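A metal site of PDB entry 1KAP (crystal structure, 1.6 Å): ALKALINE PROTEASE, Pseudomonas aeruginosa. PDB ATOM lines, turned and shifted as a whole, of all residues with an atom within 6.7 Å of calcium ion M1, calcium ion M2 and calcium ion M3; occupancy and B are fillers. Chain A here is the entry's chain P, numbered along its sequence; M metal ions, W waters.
Within 4 Å of calcium ion M2: Gly 343, Gly 345, Asp 347, Gly 360, Gly 361, Ala 362 and Asp 365.
Within 4 Å of calcium ion M3: Gly 379, Ala 380, Gly 381, Asp 383 and Asp 409.
The nearest printed residue that does not touch calcium ion M3 is Gly 378 (4.1 Å).
Calcium ion M2 is bound by O of Ala 362, O of Gly 360, O of Gly 343, OD1 of Asp 365, O of Gly 345 and OD2 of Asp 347.
Calcium ion M2 has six donor atoms within binding distance.
Slightly farther from calcium ion M2 lies OD2 of Asp 365 (3.1 Å).
Eight residues have an atom within 4 Å of calcium ion M1: Gly 361, Ala 362, Gly 363, Asp 365, Gly 378, Gly 379, Ala 380 and Asp 383.
Water W2 lies within hydrogen-bond range of OD2 of Asp 409 and OD1 of Asp 403.
Calcium ion M3 is bound by OD2 of Asp 383, water W1, O of Gly 379, water W2, O of Gly 381 and OD1 of Asp 409.
OD1 of Asp 403 sits at hydrogen-bond distance from N of Gly 378 (2.9 Å).
N of Gly 360 sits at hydrogen-bond distance from O of Trp 377, 2.8 Å away.
N of Gly 343 lies close to NE2 of Gln 310.
The side-chain carboxylate (OD2) of Asp 403 sits at hydrogen-bond distance from the backbone NH (N) of Gly 379 (2.8 Å).
The side-chain carboxylate of Asp 347 is in hydrogen-bond range of the backbone NH of Gln 310 (2.9 Å).
OD2 of Asp 409 lies within hydrogen-bond range of N of Val 405, 2.8 Å away.
Calcium ion M1 is bound by O of Gly 378, at 2.3 Å.
Calcium ion M1 is bound by O of Gly 361 (2.3 Å).
The side-chain carboxylate (OD2) of Asp 365 is bound to calcium ion M1 (2.3 Å).
O of Ala 380 binds calcium ion M1 (2.4 Å).
OD1 of Asp 383 is bound to calcium ion M1, at 2.4 Å.
The backbone carbonyl oxygen (O) of Gly 363 binds calcium ion M1, 2.4 Å away.
Calcium ion M1 has six donor atoms within binding distance.
Slightly farther from calcium ion M1 lies the side-chain carboxylate (OD2) of Asp 383 (3.1 Å).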
ATOM      1  N   GLN A 308     -26.418   9.637  11.570  1.00  0.00           N
ATOM      2  CA  GLN A 308     -26.862   8.962  12.784  1.00  0.00           C
ATOM      3  C   GLN A 308     -25.661   8.375  13.502  1.00  0.00           C
ATOM      4  O   GLN A 308     -24.592   8.189  12.906  1.00  0.00           O
ATOM      5  CB  GLN A 308     -27.834   7.816  12.448  1.00  0.00           C
ATOM      6  CG  GLN A 308     -29.100   8.210  11.707  1.00  0.00           C
ATOM      7  CD  GLN A 308     -28.951   8.168  10.196  1.00  0.00           C
ATOM      8  OE1 GLN A 308     -27.844   8.028   9.666  1.00  0.00           O
ATOM      9  NE2 GLN A 308     -30.061   8.271   9.492  1.00  0.00           N
ATOM     10  N   GLN A 310     -23.506   5.547  14.752  1.00  0.00           N
ATOM     11  CA  GLN A 310     -23.341   4.201  14.253  1.00  0.00           C
ATOM     12  C   GLN A 310     -22.450   3.329  15.118  1.00  0.00           C
ATOM     13  O   GLN A 310     -21.665   3.844  15.911  1.00  0.00           O
ATOM     14  CB  GLN A 310     -22.791   4.260  12.814  1.00  0.00           C
ATOM     15  CG  GLN A 310     -23.603   5.169  11.902  1.00  0.00           C
ATOM     16  CD  GLN A 310     -23.101   5.189  10.488  1.00  0.00           C
ATOM     17  OE1 GLN A 310     -23.504   4.362   9.670  1.00  0.00           O
ATOM     18  NE2 GLN A 310     -22.214   6.129  10.162  1.00  0.00           N
ATOM     19  N   GLY A 342     -16.492   6.076   9.783  1.00  0.00           N
ATOM     20  CA  GLY A 342     -17.745   6.463  10.415  1.00  0.00           C
ATOM     21  C   GLY A 342     -18.328   7.718   9.752  1.00  0.00           C
ATOM     22  O   GLY A 342     -17.743   8.267   8.804  1.00  0.00           O
ATOM     23  N   GLY A 343     -19.482   8.161  10.249  1.00  0.00           N
ATOM     24  CA  GLY A 343     -20.135   9.336   9.699  1.00  0.00           C
ATOM     25  C   GLY A 343     -20.017  10.527  10.627  1.00  0.00           C
ATOM     26  O   GLY A 343     -19.172  10.557  11.529  1.00  0.00           O
ATOM     27  N   SER A 344     -20.906  11.500  10.470  1.00  0.00           N
ATOM     28  CA  SER A 344     -20.850  12.688  11.315  1.00  0.00           C
ATOM     29  C   SER A 344     -21.458  12.535  12.713  1.00  0.00           C
ATOM     30  O   SER A 344     -21.447  13.480  13.508  1.00  0.00           O
ATOM     31  CB  SER A 344     -21.439  13.887  10.575  1.00  0.00           C
ATOM     32  OG  SER A 344     -22.826  13.726  10.335  1.00  0.00           O
ATOM     33  N   GLY A 345     -22.023  11.379  13.027  1.00  0.00           N
ATOM     34  CA  GLY A 345     -22.568  11.167  14.351  1.00  0.00           C
ATOM     35  C   GLY A 345     -21.485  10.656  15.284  1.00  0.00           C
ATOM     36  O   GLY A 345     -20.332  10.519  14.885  1.00  0.00           O
ATOM     37  N   SER A 346     -21.839  10.382  16.533  1.00  0.00           N
ATOM     38  CA  SER A 346     -20.893   9.841  17.504  1.00  0.00           C
ATOM     39  C   SER A 346     -20.926   8.320  17.316  1.00  0.00           C
ATOM     40  O   SER A 346     -21.898   7.653  17.660  1.00  0.00           O
ATOM     41  CB  SER A 346     -21.293  10.278  18.915  1.00  0.00           C
ATOM     42  OG  SER A 346     -21.253  11.698  18.977  1.00  0.00           O
ATOM     43  N   ASP A 347     -19.857   7.789  16.748  1.00  0.00           N
ATOM     44  CA  ASP A 347     -19.766   6.375  16.392  1.00  0.00           C
ATOM     45  C   ASP A 347     -18.891   5.508  17.262  1.00  0.00           C
ATOM     46  O   ASP A 347     -18.020   5.994  17.978  1.00  0.00           O
ATOM     47  CB  ASP A 347     -19.247   6.269  14.962  1.00  0.00           C
ATOM     48  CG  ASP A 347     -19.987   7.159  14.000  1.00  0.00           C
ATOM     49  OD1 ASP A 347     -21.234   7.154  14.018  1.00  0.00           O
ATOM     50  OD2 ASP A 347     -19.328   7.870  13.226  1.00  0.00           O
ATOM     51  N   LEU A 349     -16.402   2.376  16.638  1.00  0.00           N
ATOM     52  CA  LEU A 349     -15.695   1.624  15.599  1.00  0.00           C
ATOM     53  C   LEU A 349     -14.800   0.574  16.252  1.00  0.00           C
ATOM     54  O   LEU A 349     -13.881   0.912  17.025  1.00  0.00           O
ATOM     55  CB  LEU A 349     -14.866   2.532  14.705  1.00  0.00           C
ATOM     56  CG  LEU A 349     -15.621   3.449  13.749  1.00  0.00           C
ATOM     57  CD1 LEU A 349     -15.857   4.786  14.403  1.00  0.00           C
ATOM     58  CD2 LEU A 349     -14.798   3.647  12.507  1.00  0.00           C
ATOM     59  N   LYS A 359     -11.542   5.451  10.870  1.00  0.00           N
ATOM     60  CA  LYS A 359     -11.699   6.897  10.835  1.00  0.00           C
ATOM     61  C   LYS A 359     -13.071   7.269  11.396  1.00  0.00           C
ATOM     62  O   LYS A 359     -14.097   6.871  10.850  1.00  0.00           O
ATOM     63  CB  LYS A 359     -11.553   7.422   9.414  1.00  0.00           C
ATOM     64  CG  LYS A 359     -10.225   7.113   8.798  1.00  0.00           C
ATOM     65  CD  LYS A 359     -10.086   7.836   7.504  1.00  0.00           C
ATOM     66  CE  LYS A 359      -8.719   7.600   6.911  1.00  0.00           C
ATOM     67  NZ  LYS A 359      -8.490   8.425   5.690  1.00  0.00           N
ATOM     68  N   GLY A 360     -13.075   8.027  12.489  1.00  0.00           N
ATOM     69  CA  GLY A 360     -14.312   8.399  13.126  1.00  0.00           C
ATOM     70  C   GLY A 360     -15.091   9.506  12.460  1.00  0.00           C
ATOM     71  O   GLY A 360     -16.316   9.521  12.559  1.00  0.00           O
ATOM     72  N   GLY A 361     -14.414  10.412  11.778  1.00  0.00           N
ATOM     73  CA  GLY A 361     -15.101  11.540  11.153  1.00  0.00           C
ATOM     74  C   GLY A 361     -15.554  12.494  12.257  1.00  0.00           C
ATOM     75  O   GLY A 361     -15.024  12.452  13.371  1.00  0.00           O
ATOM     76  N   ALA A 362     -16.491  13.384  11.947  1.00  0.00           N
ATOM     77  CA  ALA A 362     -17.006  14.321  12.947  1.00  0.00           C
ATOM     78  C   ALA A 362     -17.756  13.534  14.026  1.00  0.00           C
ATOM     79  O   ALA A 362     -18.095  12.364  13.826  1.00  0.00           O
ATOM     80  CB  ALA A 362     -17.927  15.359  12.285  1.00  0.00           C
ATOM     81  N   GLY A 363     -18.050  14.184  15.138  1.00  0.00           N
ATOM     82  CA  GLY A 363     -18.749  13.529  16.226  1.00  0.00           C
ATOM     83  C   GLY A 363     -17.750  12.993  17.235  1.00  0.00           C
ATOM     84  O   GLY A 363     -16.565  12.883  16.942  1.00  0.00           O
ATOM     85  N   ASN A 364     -18.226  12.682  18.422  1.00  0.00           N
ATOM     86  CA  ASN A 364     -17.401  12.148  19.501  1.00  0.00           C
ATOM     87  C   ASN A 364     -17.401  10.628  19.388  1.00  0.00           C
ATOM     88  O   ASN A 364     -18.268   9.942  19.924  1.00  0.00           O
ATOM     89  CB  ASN A 364     -17.949  12.593  20.863  1.00  0.00           C
ATOM     90  CG  ASN A 364     -17.853  14.110  21.071  1.00  0.00           C
ATOM     91  OD1 ASN A 364     -17.269  14.853  20.273  1.00  0.00           O
ATOM     92  ND2 ASN A 364     -18.432  14.573  22.159  1.00  0.00           N
ATOM     93  N   ASP A 365     -16.398  10.108  18.692  1.00  0.00           N
ATOM     94  CA  ASP A 365     -16.288   8.690  18.417  1.00  0.00           C
ATOM     95  C   ASP A 365     -15.460   7.907  19.419  1.00  0.00           C
ATOM     96  O   ASP A 365     -14.605   8.471  20.110  1.00  0.00           O
ATOM     97  CB  ASP A 365     -15.707   8.505  17.016  1.00  0.00           C
ATOM     98  CG  ASP A 365     -16.433   9.347  15.974  1.00  0.00           C
ATOM     99  OD1 ASP A 365     -17.614   9.083  15.706  1.00  0.00           O
ATOM    100  OD2 ASP A 365     -15.820  10.274  15.420  1.00  0.00           O
ATOM    101  N   LEU A 367     -13.051   4.557  19.398  1.00  0.00           N
ATOM    102  CA  LEU A 367     -12.345   3.657  18.494  1.00  0.00           C
ATOM    103  C   LEU A 367     -11.595   2.584  19.268  1.00  0.00           C
ATOM    104  O   LEU A 367     -10.970   2.853  20.289  1.00  0.00           O
ATOM    105  CB  LEU A 367     -11.371   4.461  17.584  1.00  0.00           C
ATOM    106  CG  LEU A 367     -11.969   5.457  16.565  1.00  0.00           C
ATOM    107  CD1 LEU A 367     -12.254   6.800  17.256  1.00  0.00           C
ATOM    108  CD2 LEU A 367     -11.002   5.694  15.424  1.00  0.00           C
ATOM    109  N   TRP A 377      -7.811   7.384  13.352  1.00  0.00           N
ATOM    110  CA  TRP A 377      -8.119   8.785  13.109  1.00  0.00           C
ATOM    111  C   TRP A 377      -9.420   9.108  13.830  1.00  0.00           C
ATOM    112  O   TRP A 377     -10.465   8.553  13.487  1.00  0.00           O
ATOM    113  CB  TRP A 377      -8.325   9.015  11.632  1.00  0.00           C
ATOM    114  CG  TRP A 377      -7.184   8.640  10.773  1.00  0.00           C
ATOM    115  CD1 TRP A 377      -6.815   7.367  10.353  1.00  0.00           C
ATOM    116  CD2 TRP A 377      -6.280   9.537  10.146  1.00  0.00           C
ATOM    117  NE1 TRP A 377      -5.757   7.448   9.493  1.00  0.00           N
ATOM    118  CE2 TRP A 377      -5.402   8.766   9.343  1.00  0.00           C
ATOM    119  CE3 TRP A 377      -6.143  10.928  10.166  1.00  0.00           C
ATOM    120  CZ2 TRP A 377      -4.394   9.340   8.577  1.00  0.00           C
ATOM    121  CZ3 TRP A 377      -5.138  11.502   9.410  1.00  0.00           C
ATOM    122  CH2 TRP A 377      -4.280  10.713   8.621  1.00  0.00           C
ATOM    123  N   GLY A 378      -9.378   9.993  14.824  1.00  0.00           N
ATOM    124  CA  GLY A 378     -10.595  10.358  15.510  1.00  0.00           C
ATOM    125  C   GLY A 378     -11.420  11.389  14.743  1.00  0.00           C
ATOM    126  O   GLY A 378     -12.649  11.413  14.841  1.00  0.00           O
ATOM    127  N   GLY A 379     -10.749  12.187  13.921  1.00  0.00           N
ATOM    128  CA  GLY A 379     -11.426  13.251  13.183  1.00  0.00           C
ATOM    129  C   GLY A 379     -11.817  14.367  14.152  1.00  0.00           C
ATOM    130  O   GLY A 379     -11.289  14.455  15.266  1.00  0.00           O
ATOM    131  N   ALA A 380     -12.721  15.245  13.726  1.00  0.00           N
ATOM    132  CA  ALA A 380     -13.180  16.340  14.587  1.00  0.00           C
ATOM    133  C   ALA A 380     -13.941  15.757  15.761  1.00  0.00           C
ATOM    134  O   ALA A 380     -14.416  14.625  15.706  1.00  0.00           O
ATOM    135  CB  ALA A 380     -14.082  17.282  13.794  1.00  0.00           C
ATOM    136  N   GLY A 381     -14.070  16.535  16.823  1.00  0.00           N
ATOM    137  CA  GLY A 381     -14.788  16.080  18.002  1.00  0.00           C
ATOM    138  C   GLY A 381     -13.869  15.457  19.026  1.00  0.00           C
ATOM    139  O   GLY A 381     -12.679  15.256  18.776  1.00  0.00           O
ATOM    140  N   ALA A 382     -14.420  15.169  20.199  1.00  0.00           N
ATOM    141  CA  ALA A 382     -13.674  14.571  21.293  1.00  0.00           C
ATOM    142  C   ALA A 382     -13.727  13.036  21.152  1.00  0.00           C
ATOM    143  O   ALA A 382     -14.727  12.405  21.529  1.00  0.00           O
ATOM    144  CB  ALA A 382     -14.276  15.010  22.616  1.00  0.00           C
ATOM    145  N   ASP A 383     -12.649  12.462  20.649  1.00  0.00           N
ATOM    146  CA  ASP A 383     -12.588  11.019  20.420  1.00  0.00           C
ATOM    147  C   ASP A 383     -11.821  10.251  21.476  1.00  0.00           C
ATOM    148  O   ASP A 383     -10.875  10.763  22.070  1.00  0.00           O
ATOM    149  CB  ASP A 383     -12.012  10.779  19.038  1.00  0.00           C
ATOM    150  CG  ASP A 383     -12.736  11.599  17.986  1.00  0.00           C
ATOM    151  OD1 ASP A 383     -13.930  11.344  17.745  1.00  0.00           O
ATOM    152  OD2 ASP A 383     -12.124  12.535  17.421  1.00  0.00           O
ATOM    153  N   PHE A 385      -9.747   6.665  22.258  1.00  0.00           N
ATOM    154  CA  PHE A 385      -9.062   5.497  21.713  1.00  0.00           C
ATOM    155  C   PHE A 385      -8.939   4.505  22.869  1.00  0.00           C
ATOM    156  O   PHE A 385      -8.245   4.755  23.850  1.00  0.00           O
ATOM    157  CB  PHE A 385      -7.714   5.920  21.132  1.00  0.00           C
ATOM    158  CG  PHE A 385      -7.842   7.015  20.123  1.00  0.00           C
ATOM    159  CD1 PHE A 385      -8.058   6.722  18.773  1.00  0.00           C
ATOM    160  CD2 PHE A 385      -7.812   8.365  20.518  1.00  0.00           C
ATOM    161  CE1 PHE A 385      -8.256   7.743  17.835  1.00  0.00           C
ATOM    162  CE2 PHE A 385      -8.013   9.385  19.589  1.00  0.00           C
ATOM    163  CZ  PHE A 385      -8.237   9.079  18.247  1.00  0.00           C
ATOM    164  N   ASP A 403      -4.191  11.779  14.448  1.00  0.00           N
ATOM    165  CA  ASP A 403      -4.647  13.160  14.535  1.00  0.00           C
ATOM    166  C   ASP A 403      -5.053  13.520  15.964  1.00  0.00           C
ATOM    167  O   ASP A 403      -6.055  14.201  16.198  1.00  0.00           O
ATOM    168  CB  ASP A 403      -5.833  13.372  13.564  1.00  0.00           C
ATOM    169  CG  ASP A 403      -7.065  12.498  13.904  1.00  0.00           C
ATOM    170  OD1 ASP A 403      -7.018  11.651  14.815  1.00  0.00           O
ATOM    171  OD2 ASP A 403      -8.106  12.668  13.244  1.00  0.00           O
ATOM    172  N   PHE A 404      -4.248  13.071  16.921  1.00  0.00           N
ATOM    173  CA  PHE A 404      -4.536  13.301  18.313  1.00  0.00           C
ATOM    174  C   PHE A 404      -4.496  14.775  18.713  1.00  0.00           C
ATOM    175  O   PHE A 404      -3.543  15.483  18.406  1.00  0.00           O
ATOM    176  CB  PHE A 404      -3.570  12.506  19.193  1.00  0.00           C
ATOM    177  CG  PHE A 404      -4.033  12.350  20.608  1.00  0.00           C
ATOM    178  CD1 PHE A 404      -4.881  11.300  20.967  1.00  0.00           C
ATOM    179  CD2 PHE A 404      -3.650  13.277  21.589  1.00  0.00           C
ATOM    180  CE1 PHE A 404      -5.345  11.174  22.276  1.00  0.00           C
ATOM    181  CE2 PHE A 404      -4.108  13.151  22.879  1.00  0.00           C
ATOM    182  CZ  PHE A 404      -4.955  12.101  23.239  1.00  0.00           C
ATOM    183  N   VAL A 405      -5.532  15.217  19.408  1.00  0.00           N
ATOM    184  CA  VAL A 405      -5.609  16.605  19.862  1.00  0.00           C
ATOM    185  C   VAL A 405      -5.753  16.628  21.385  1.00  0.00           C
ATOM    186  O   VAL A 405      -6.791  16.232  21.931  1.00  0.00           O
ATOM    187  CB  VAL A 405      -6.804  17.346  19.222  1.00  0.00           C
ATOM    188  CG1 VAL A 405      -6.911  18.756  19.772  1.00  0.00           C
ATOM    189  CG2 VAL A 405      -6.643  17.376  17.716  1.00  0.00           C
ATOM    190  N   GLN A 408      -8.835  17.360  23.964  1.00  0.00           N
ATOM    191  CA  GLN A 408     -10.072  16.976  23.275  1.00  0.00           C
ATOM    192  C   GLN A 408     -10.179  15.455  23.243  1.00  0.00           C
ATOM    193  O   GLN A 408     -11.136  14.894  23.772  1.00  0.00           O
ATOM    194  CB  GLN A 408     -10.118  17.519  21.855  1.00  0.00           C
ATOM    195  CG  GLN A 408     -11.060  18.710  21.694  1.00  0.00           C
ATOM    196  CD  GLN A 408     -11.716  18.742  20.318  1.00  0.00           C
ATOM    197  OE1 GLN A 408     -11.030  18.680  19.290  1.00  0.00           O
ATOM    198  NE2 GLN A 408     -13.041  18.841  20.290  1.00  0.00           N
ATOM    199  N   ASP A 409      -9.197  14.807  22.644  1.00  0.00           N
ATOM    200  CA  ASP A 409      -9.200  13.345  22.562  1.00  0.00           C
ATOM    201  C   ASP A 409      -8.654  12.719  23.842  1.00  0.00           C
ATOM    202  O   ASP A 409      -8.039  13.407  24.666  1.00  0.00           O
ATOM    203  CB  ASP A 409      -8.373  12.873  21.366  1.00  0.00           C
ATOM    204  CG  ASP A 409      -8.832  13.477  20.062  1.00  0.00           C
ATOM    205  OD1 ASP A 409     -10.044  13.665  19.852  1.00  0.00           O
ATOM    206  OD2 ASP A 409      -7.967  13.755  19.236  1.00  0.00           O
HETATM  207 CA    CA M   1     -14.623  12.276  15.662  1.00  0.00          CA
HETATM  208 CA    CA M   2     -18.321  10.046  13.660  1.00  0.00          CA
HETATM  209 CA    CA M   3     -10.755  14.326  17.580  1.00  0.00          CA
HETATM  210  O   HOH W   1     -10.111  16.574  17.452  1.00  0.00           O
HETATM  211  O   HOH W   2      -8.841  13.015  16.861  1.00  0.00           O
